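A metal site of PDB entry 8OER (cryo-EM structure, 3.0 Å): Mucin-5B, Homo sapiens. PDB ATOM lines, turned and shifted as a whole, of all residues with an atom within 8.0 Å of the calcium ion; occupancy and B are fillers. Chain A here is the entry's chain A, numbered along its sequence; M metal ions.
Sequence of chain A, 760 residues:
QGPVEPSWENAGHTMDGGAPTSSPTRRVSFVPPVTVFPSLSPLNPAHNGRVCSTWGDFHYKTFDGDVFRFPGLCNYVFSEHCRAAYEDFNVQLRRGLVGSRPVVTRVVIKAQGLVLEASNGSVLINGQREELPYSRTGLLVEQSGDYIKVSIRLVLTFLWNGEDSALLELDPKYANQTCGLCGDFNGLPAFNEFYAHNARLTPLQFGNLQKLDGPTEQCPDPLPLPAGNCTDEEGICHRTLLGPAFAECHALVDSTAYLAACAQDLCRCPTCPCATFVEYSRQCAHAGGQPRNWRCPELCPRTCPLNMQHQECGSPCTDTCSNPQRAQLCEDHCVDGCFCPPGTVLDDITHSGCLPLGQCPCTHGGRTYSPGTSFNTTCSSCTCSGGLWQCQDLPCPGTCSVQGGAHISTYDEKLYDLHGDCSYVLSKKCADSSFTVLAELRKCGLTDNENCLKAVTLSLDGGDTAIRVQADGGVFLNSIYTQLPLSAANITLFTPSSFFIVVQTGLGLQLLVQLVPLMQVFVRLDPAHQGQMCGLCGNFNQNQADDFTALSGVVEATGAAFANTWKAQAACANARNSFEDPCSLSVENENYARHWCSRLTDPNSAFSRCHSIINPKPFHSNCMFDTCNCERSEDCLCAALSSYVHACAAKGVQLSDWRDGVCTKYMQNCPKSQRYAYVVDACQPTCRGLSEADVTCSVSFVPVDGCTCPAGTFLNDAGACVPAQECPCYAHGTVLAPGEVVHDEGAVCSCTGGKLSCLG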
ATOM      1  N   THR A  62      30.295  -5.809  -6.193  1.00  0.00           N
ATOM      2  CA  THR A  62      29.713  -7.013  -5.641  1.00  0.00           C
ATOM      3  C   THR A  62      28.375  -7.309  -6.302  1.00  0.00           C
ATOM      4  O   THR A  62      27.885  -6.558  -7.146  1.00  0.00           O
ATOM      5  CB  THR A  62      29.534  -6.881  -4.129  1.00  0.00           C
ATOM      6  OG1 THR A  62      28.248  -6.304  -3.848  1.00  0.00           O
ATOM      7  CG2 THR A  62      30.628  -6.024  -3.523  1.00  0.00           C
ATOM      8  N   PHE A  63      27.759  -8.425  -5.905  1.00  0.00           N
ATOM      9  CA  PHE A  63      26.514  -8.852  -6.535  1.00  0.00           C
ATOM     10  C   PHE A  63      25.416  -7.818  -6.343  1.00  0.00           C
ATOM     11  O   PHE A  63      24.652  -7.535  -7.280  1.00  0.00           O
ATOM     12  CB  PHE A  63      26.056 -10.187  -5.954  1.00  0.00           C
ATOM     13  CG  PHE A  63      26.986 -11.317  -6.243  1.00  0.00           C
ATOM     14  CD1 PHE A  63      27.532 -11.479  -7.497  1.00  0.00           C
ATOM     15  CD2 PHE A  63      27.278 -12.236  -5.261  1.00  0.00           C
ATOM     16  CE1 PHE A  63      28.374 -12.531  -7.758  1.00  0.00           C
ATOM     17  CE2 PHE A  63      28.115 -13.289  -5.508  1.00  0.00           C
ATOM     18  CZ  PHE A  63      28.670 -13.431  -6.764  1.00  0.00           C
ATOM     19  N   ASP A  64      25.308  -7.249  -5.154  1.00  0.00           N
ATOM     20  CA  ASP A  64      24.130  -6.486  -4.757  1.00  0.00           C
ATOM     21  C   ASP A  64      24.224  -5.014  -5.137  1.00  0.00           C
ATOM     22  O   ASP A  64      23.283  -4.263  -4.872  1.00  0.00           O
ATOM     23  CB  ASP A  64      23.900  -6.645  -3.260  1.00  0.00           C
ATOM     24  CG  ASP A  64      24.507  -7.910  -2.717  1.00  0.00           C
ATOM     25  OD1 ASP A  64      24.406  -8.957  -3.398  1.00  0.00           O
ATOM     26  OD2 ASP A  64      25.084  -7.873  -1.611  1.00  0.00           O
ATOM     27  N   ASP A  66      27.281  -2.881  -4.722  1.00  0.00           N
ATOM     28  CA  ASP A  66      28.344  -2.093  -4.140  1.00  0.00           C
ATOM     29  C   ASP A  66      29.506  -1.925  -5.113  1.00  0.00           C
ATOM     30  O   ASP A  66      29.707  -2.738  -6.017  1.00  0.00           O
ATOM     31  CB  ASP A  66      28.843  -2.726  -2.849  1.00  0.00           C
ATOM     32  CG  ASP A  66      27.803  -2.688  -1.776  1.00  0.00           C
ATOM     33  OD1 ASP A  66      26.658  -2.310  -2.083  1.00  0.00           O
ATOM     34  OD2 ASP A  66      28.114  -3.045  -0.632  1.00  0.00           O
ATOM     35  N   ASN A 176      23.251 -16.182  -0.720  1.00  0.00           N
ATOM     36  CA  ASN A 176      23.472 -16.235   0.725  1.00  0.00           C
ATOM     37  C   ASN A 176      24.483 -17.310   1.131  1.00  0.00           C
ATOM     38  O   ASN A 176      24.831 -17.408   2.304  1.00  0.00           O
ATOM     39  CB  ASN A 176      22.161 -16.462   1.465  1.00  0.00           C
ATOM     40  CG  ASN A 176      22.077 -15.678   2.753  1.00  0.00           C
ATOM     41  OD1 ASN A 176      23.049 -15.062   3.180  1.00  0.00           O
ATOM     42  ND2 ASN A 176      20.908 -15.708   3.378  1.00  0.00           N
ATOM     43  N   CYS A 182      33.182 -10.625  -4.049  1.00  0.00           N
ATOM     44  CA  CYS A 182      31.907 -10.459  -4.736  1.00  0.00           C
ATOM     45  C   CYS A 182      30.732 -10.366  -3.777  1.00  0.00           C
ATOM     46  O   CYS A 182      29.615 -10.100  -4.232  1.00  0.00           O
ATOM     47  CB  CYS A 182      31.676 -11.601  -5.736  1.00  0.00           C
ATOM     48  SG  CYS A 182      32.768 -11.589  -7.176  1.00  0.00           S
ATOM     49  N   GLY A 183      30.934 -10.590  -2.495  1.00  0.00           N
ATOM     50  CA  GLY A 183      29.875 -10.357  -1.533  1.00  0.00           C
ATOM     51  C   GLY A 183      29.186 -11.617  -1.059  1.00  0.00           C
ATOM     52  O   GLY A 183      29.785 -12.693  -1.099  1.00  0.00           O
ATOM     53  N   ASP A 184      27.936 -11.498  -0.620  1.00  0.00           N
ATOM     54  CA  ASP A 184      27.210 -12.660  -0.125  1.00  0.00           C
ATOM     55  C   ASP A 184      26.025 -13.066  -0.974  1.00  0.00           C
ATOM     56  O   ASP A 184      25.440 -14.115  -0.706  1.00  0.00           O
ATOM     57  CB  ASP A 184      26.701 -12.417   1.302  1.00  0.00           C
ATOM     58  CG  ASP A 184      26.009 -11.087   1.448  1.00  0.00           C
ATOM     59  OD1 ASP A 184      25.546 -10.567   0.419  1.00  0.00           O
ATOM     60  OD2 ASP A 184      25.905 -10.586   2.589  1.00  0.00           O
ATOM     61  N   PHE A 185      25.621 -12.266  -1.971  1.00  0.00           N
ATOM     62  CA  PHE A 185      24.515 -12.619  -2.862  1.00  0.00           C
ATOM     63  C   PHE A 185      23.194 -12.757  -2.113  1.00  0.00           C
ATOM     64  O   PHE A 185      22.315 -13.523  -2.511  1.00  0.00           O
ATOM     65  CB  PHE A 185      24.830 -13.888  -3.650  1.00  0.00           C
ATOM     66  CG  PHE A 185      24.041 -14.049  -4.913  1.00  0.00           C
ATOM     67  CD1 PHE A 185      23.256 -13.028  -5.404  1.00  0.00           C
ATOM     68  CD2 PHE A 185      24.095 -15.234  -5.621  1.00  0.00           C
ATOM     69  CE1 PHE A 185      22.535 -13.184  -6.554  1.00  0.00           C
ATOM     70  CE2 PHE A 185      23.370 -15.400  -6.780  1.00  0.00           C
ATOM     71  CZ  PHE A 185      22.593 -14.370  -7.253  1.00  0.00           C
ATOM     72  N   ASN A 186      23.043 -12.003  -1.016  1.00  0.00           N
ATOM     73  CA  ASN A 186      21.781 -11.959  -0.294  1.00  0.00           C
ATOM     74  C   ASN A 186      20.851 -10.877  -0.820  1.00  0.00           C
ATOM     75  O   ASN A 186      19.702 -10.788  -0.371  1.00  0.00           O
ATOM     76  CB  ASN A 186      22.025 -11.733   1.198  1.00  0.00           C
ATOM     77  CG  ASN A 186      22.754 -10.441   1.478  1.00  0.00           C
ATOM     78  OD1 ASN A 186      23.040  -9.661   0.573  1.00  0.00           O
ATOM     79  ND2 ASN A 186      23.068 -10.203   2.746  1.00  0.00           N
ATOM     80  N   GLY A 187      21.321 -10.045  -1.745  1.00  0.00           N
ATOM     81  CA  GLY A 187      20.525  -8.999  -2.339  1.00  0.00           C
ATOM     82  C   GLY A 187      20.576  -7.662  -1.656  1.00  0.00           C
ATOM     83  O   GLY A 187      20.130  -6.663  -2.246  1.00  0.00           O
ATOM     84  N   LEU A 188      21.127  -7.589  -0.451  1.00  0.00           N
ATOM     85  CA  LEU A 188      21.183  -6.335   0.291  1.00  0.00           C
ATOM     86  C   LEU A 188      22.572  -5.738   0.155  1.00  0.00           C
ATOM     87  O   LEU A 188      23.530  -6.243   0.762  1.00  0.00           O
ATOM     88  CB  LEU A 188      20.847  -6.563   1.764  1.00  0.00           C
ATOM     89  CG  LEU A 188      19.416  -7.065   1.988  1.00  0.00           C
ATOM     90  CD1 LEU A 188      19.238  -7.560   3.405  1.00  0.00           C
ATOM     91  CD2 LEU A 188      18.429  -5.956   1.694  1.00  0.00           C
ATOM     92  N   PRO A 189      22.734  -4.666  -0.609  1.00  0.00           N
ATOM     93  CA  PRO A 189      24.072  -4.170  -0.924  1.00  0.00           C
ATOM     94  C   PRO A 189      24.794  -3.555   0.258  1.00  0.00           C
ATOM     95  O   PRO A 189      25.896  -3.976   0.614  1.00  0.00           O
ATOM     96  CB  PRO A 189      23.822  -3.115  -2.005  1.00  0.00           C
ATOM     97  CG  PRO A 189      22.392  -2.797  -1.959  1.00  0.00           C
ATOM     98  CD  PRO A 189      21.666  -3.898  -1.277  1.00  0.00           C
ATOM     99  N   ALA A 190      24.172  -2.570   0.889  1.00  0.00           N
ATOM    100  CA  ALA A 190      24.885  -1.627   1.733  1.00  0.00           C
ATOM    101  C   ALA A 190      25.000  -2.071   3.182  1.00  0.00           C
ATOM    102  O   ALA A 190      25.491  -1.289   4.002  1.00  0.00           O
ATOM    103  CB  ALA A 190      24.204  -0.257   1.671  1.00  0.00           C
ATOM    104  N   PHE A 191      24.567  -3.284   3.542  1.00  0.00           N
ATOM    105  CA  PHE A 191      24.373  -3.519   4.966  1.00  0.00           C
ATOM    106  C   PHE A 191      25.089  -4.789   5.431  1.00  0.00           C
ATOM    107  O   PHE A 191      25.450  -4.887   6.609  1.00  0.00           O
ATOM    108  CB  PHE A 191      22.847  -3.564   5.252  1.00  0.00           C
ATOM    109  CG  PHE A 191      22.430  -4.399   6.436  1.00  0.00           C
ATOM    110  CD1 PHE A 191      21.319  -5.213   6.339  1.00  0.00           C
ATOM    111  CD2 PHE A 191      23.005  -4.218   7.680  1.00  0.00           C
ATOM    112  CE1 PHE A 191      20.891  -5.942   7.425  1.00  0.00           C
ATOM    113  CE2 PHE A 191      22.600  -4.958   8.767  1.00  0.00           C
ATOM    114  CZ  PHE A 191      21.531  -5.810   8.639  1.00  0.00           C
ATOM    115  N   ASN A 192      25.384  -5.733   4.536  1.00  0.00           N
ATOM    116  CA  ASN A 192      25.848  -6.999   5.074  1.00  0.00           C
ATOM    117  C   ASN A 192      27.215  -7.464   4.580  1.00  0.00           C
ATOM    118  O   ASN A 192      27.733  -8.486   5.053  1.00  0.00           O
ATOM    119  CB  ASN A 192      24.818  -8.083   4.788  1.00  0.00           C
ATOM    120  CG  ASN A 192      24.963  -9.260   5.711  1.00  0.00           C
ATOM    121  OD1 ASN A 192      25.398  -9.115   6.849  1.00  0.00           O
ATOM    122  ND2 ASN A 192      24.611 -10.440   5.226  1.00  0.00           N
ATOM    123  N   GLU A 193      27.846  -6.722   3.670  1.00  0.00           N
ATOM    124  CA  GLU A 193      29.175  -7.140   3.217  1.00  0.00           C
ATOM    125  C   GLU A 193      30.267  -6.712   4.182  1.00  0.00           C
ATOM    126  O   GLU A 193      31.299  -7.380   4.274  1.00  0.00           O
ATOM    127  CB  GLU A 193      29.499  -6.557   1.842  1.00  0.00           C
ATOM    128  CG  GLU A 193      28.571  -6.936   0.703  1.00  0.00           C
ATOM    129  CD  GLU A 193      27.839  -8.233   0.912  1.00  0.00           C
ATOM    130  OE1 GLU A 193      26.588  -8.209   0.848  1.00  0.00           O
ATOM    131  OE2 GLU A 193      28.489  -9.280   1.101  1.00  0.00           O
ATOM    132  N   PHE A 194      30.051  -5.609   4.911  1.00  0.00           N
ATOM    133  CA  PHE A 194      31.088  -4.940   5.683  1.00  0.00           C
ATOM    134  C   PHE A 194      30.733  -4.868   7.156  1.00  0.00           C
ATOM    135  O   PHE A 194      30.826  -3.807   7.765  1.00  0.00           O
ATOM    136  CB  PHE A 194      31.355  -3.539   5.141  1.00  0.00           C
ATOM    137  CG  PHE A 194      31.112  -3.416   3.676  1.00  0.00           C
ATOM    138  CD1 PHE A 194      29.857  -3.080   3.206  1.00  0.00           C
ATOM    139  CD2 PHE A 194      32.131  -3.643   2.775  1.00  0.00           C
ATOM    140  CE1 PHE A 194      29.633  -2.962   1.863  1.00  0.00           C
ATOM    141  CE2 PHE A 194      31.907  -3.525   1.432  1.00  0.00           C
ATOM    142  CZ  PHE A 194      30.656  -3.190   0.971  1.00  0.00           C
HETATM  143 CA    CA M   1      24.524  -8.177   1.512  1.00  0.00          CA
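The side-chain carboxylate (OD2) of Asp 184 sits at hydrogen-bond distance from the side-chain amide nitrogen (ND2) of Asn 192 (2.9 Å).
ND2 of Asn 186 lies close to ND2 of Asn 192, at 2.9 Å.
The side-chain hydroxyl of Thr 62 sits close to the backbone NH of Asp 64, at 3.4 Å.
The side-chain amide oxygen (OD1) of Asn 186 lies close to the side-chain carboxylate (OD2) of Asp 64, 3.5 Å away.
The backbone carbonyl oxygen (O) of Asp 184 is in hydrogen-bond range of the backbone NH (N) of Asn 176 (3.0 Å).
Asp 64 touches the calcium ion.
CB of Asn 192 touches the calcium ion, at 3.3 Å.
The nearest printed residue that does not touch the calcium ion is Pro 189 (4.5 Å).
OE1 of Glu 193 binds the calcium ion, at 2.2 Å.
OD1 of Asn 186 is bound to the calcium ion (2.3 Å).
The backbone carbonyl oxygen (O) of Leu 188 is bound to the calcium ion (2.3 Å).
The side-chain amide nitrogen (ND2) of Asn 186 is bound to the calcium ion (2.8 Å).
The calcium ion is bound by OD1 of Asp 184, 2.8 Å away.
The calcium ion has five donor atoms within binding distance.
Slightly farther from the calcium ion lies the side-chain carboxylate (OD2) of Asp 184 (3.0 Å).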
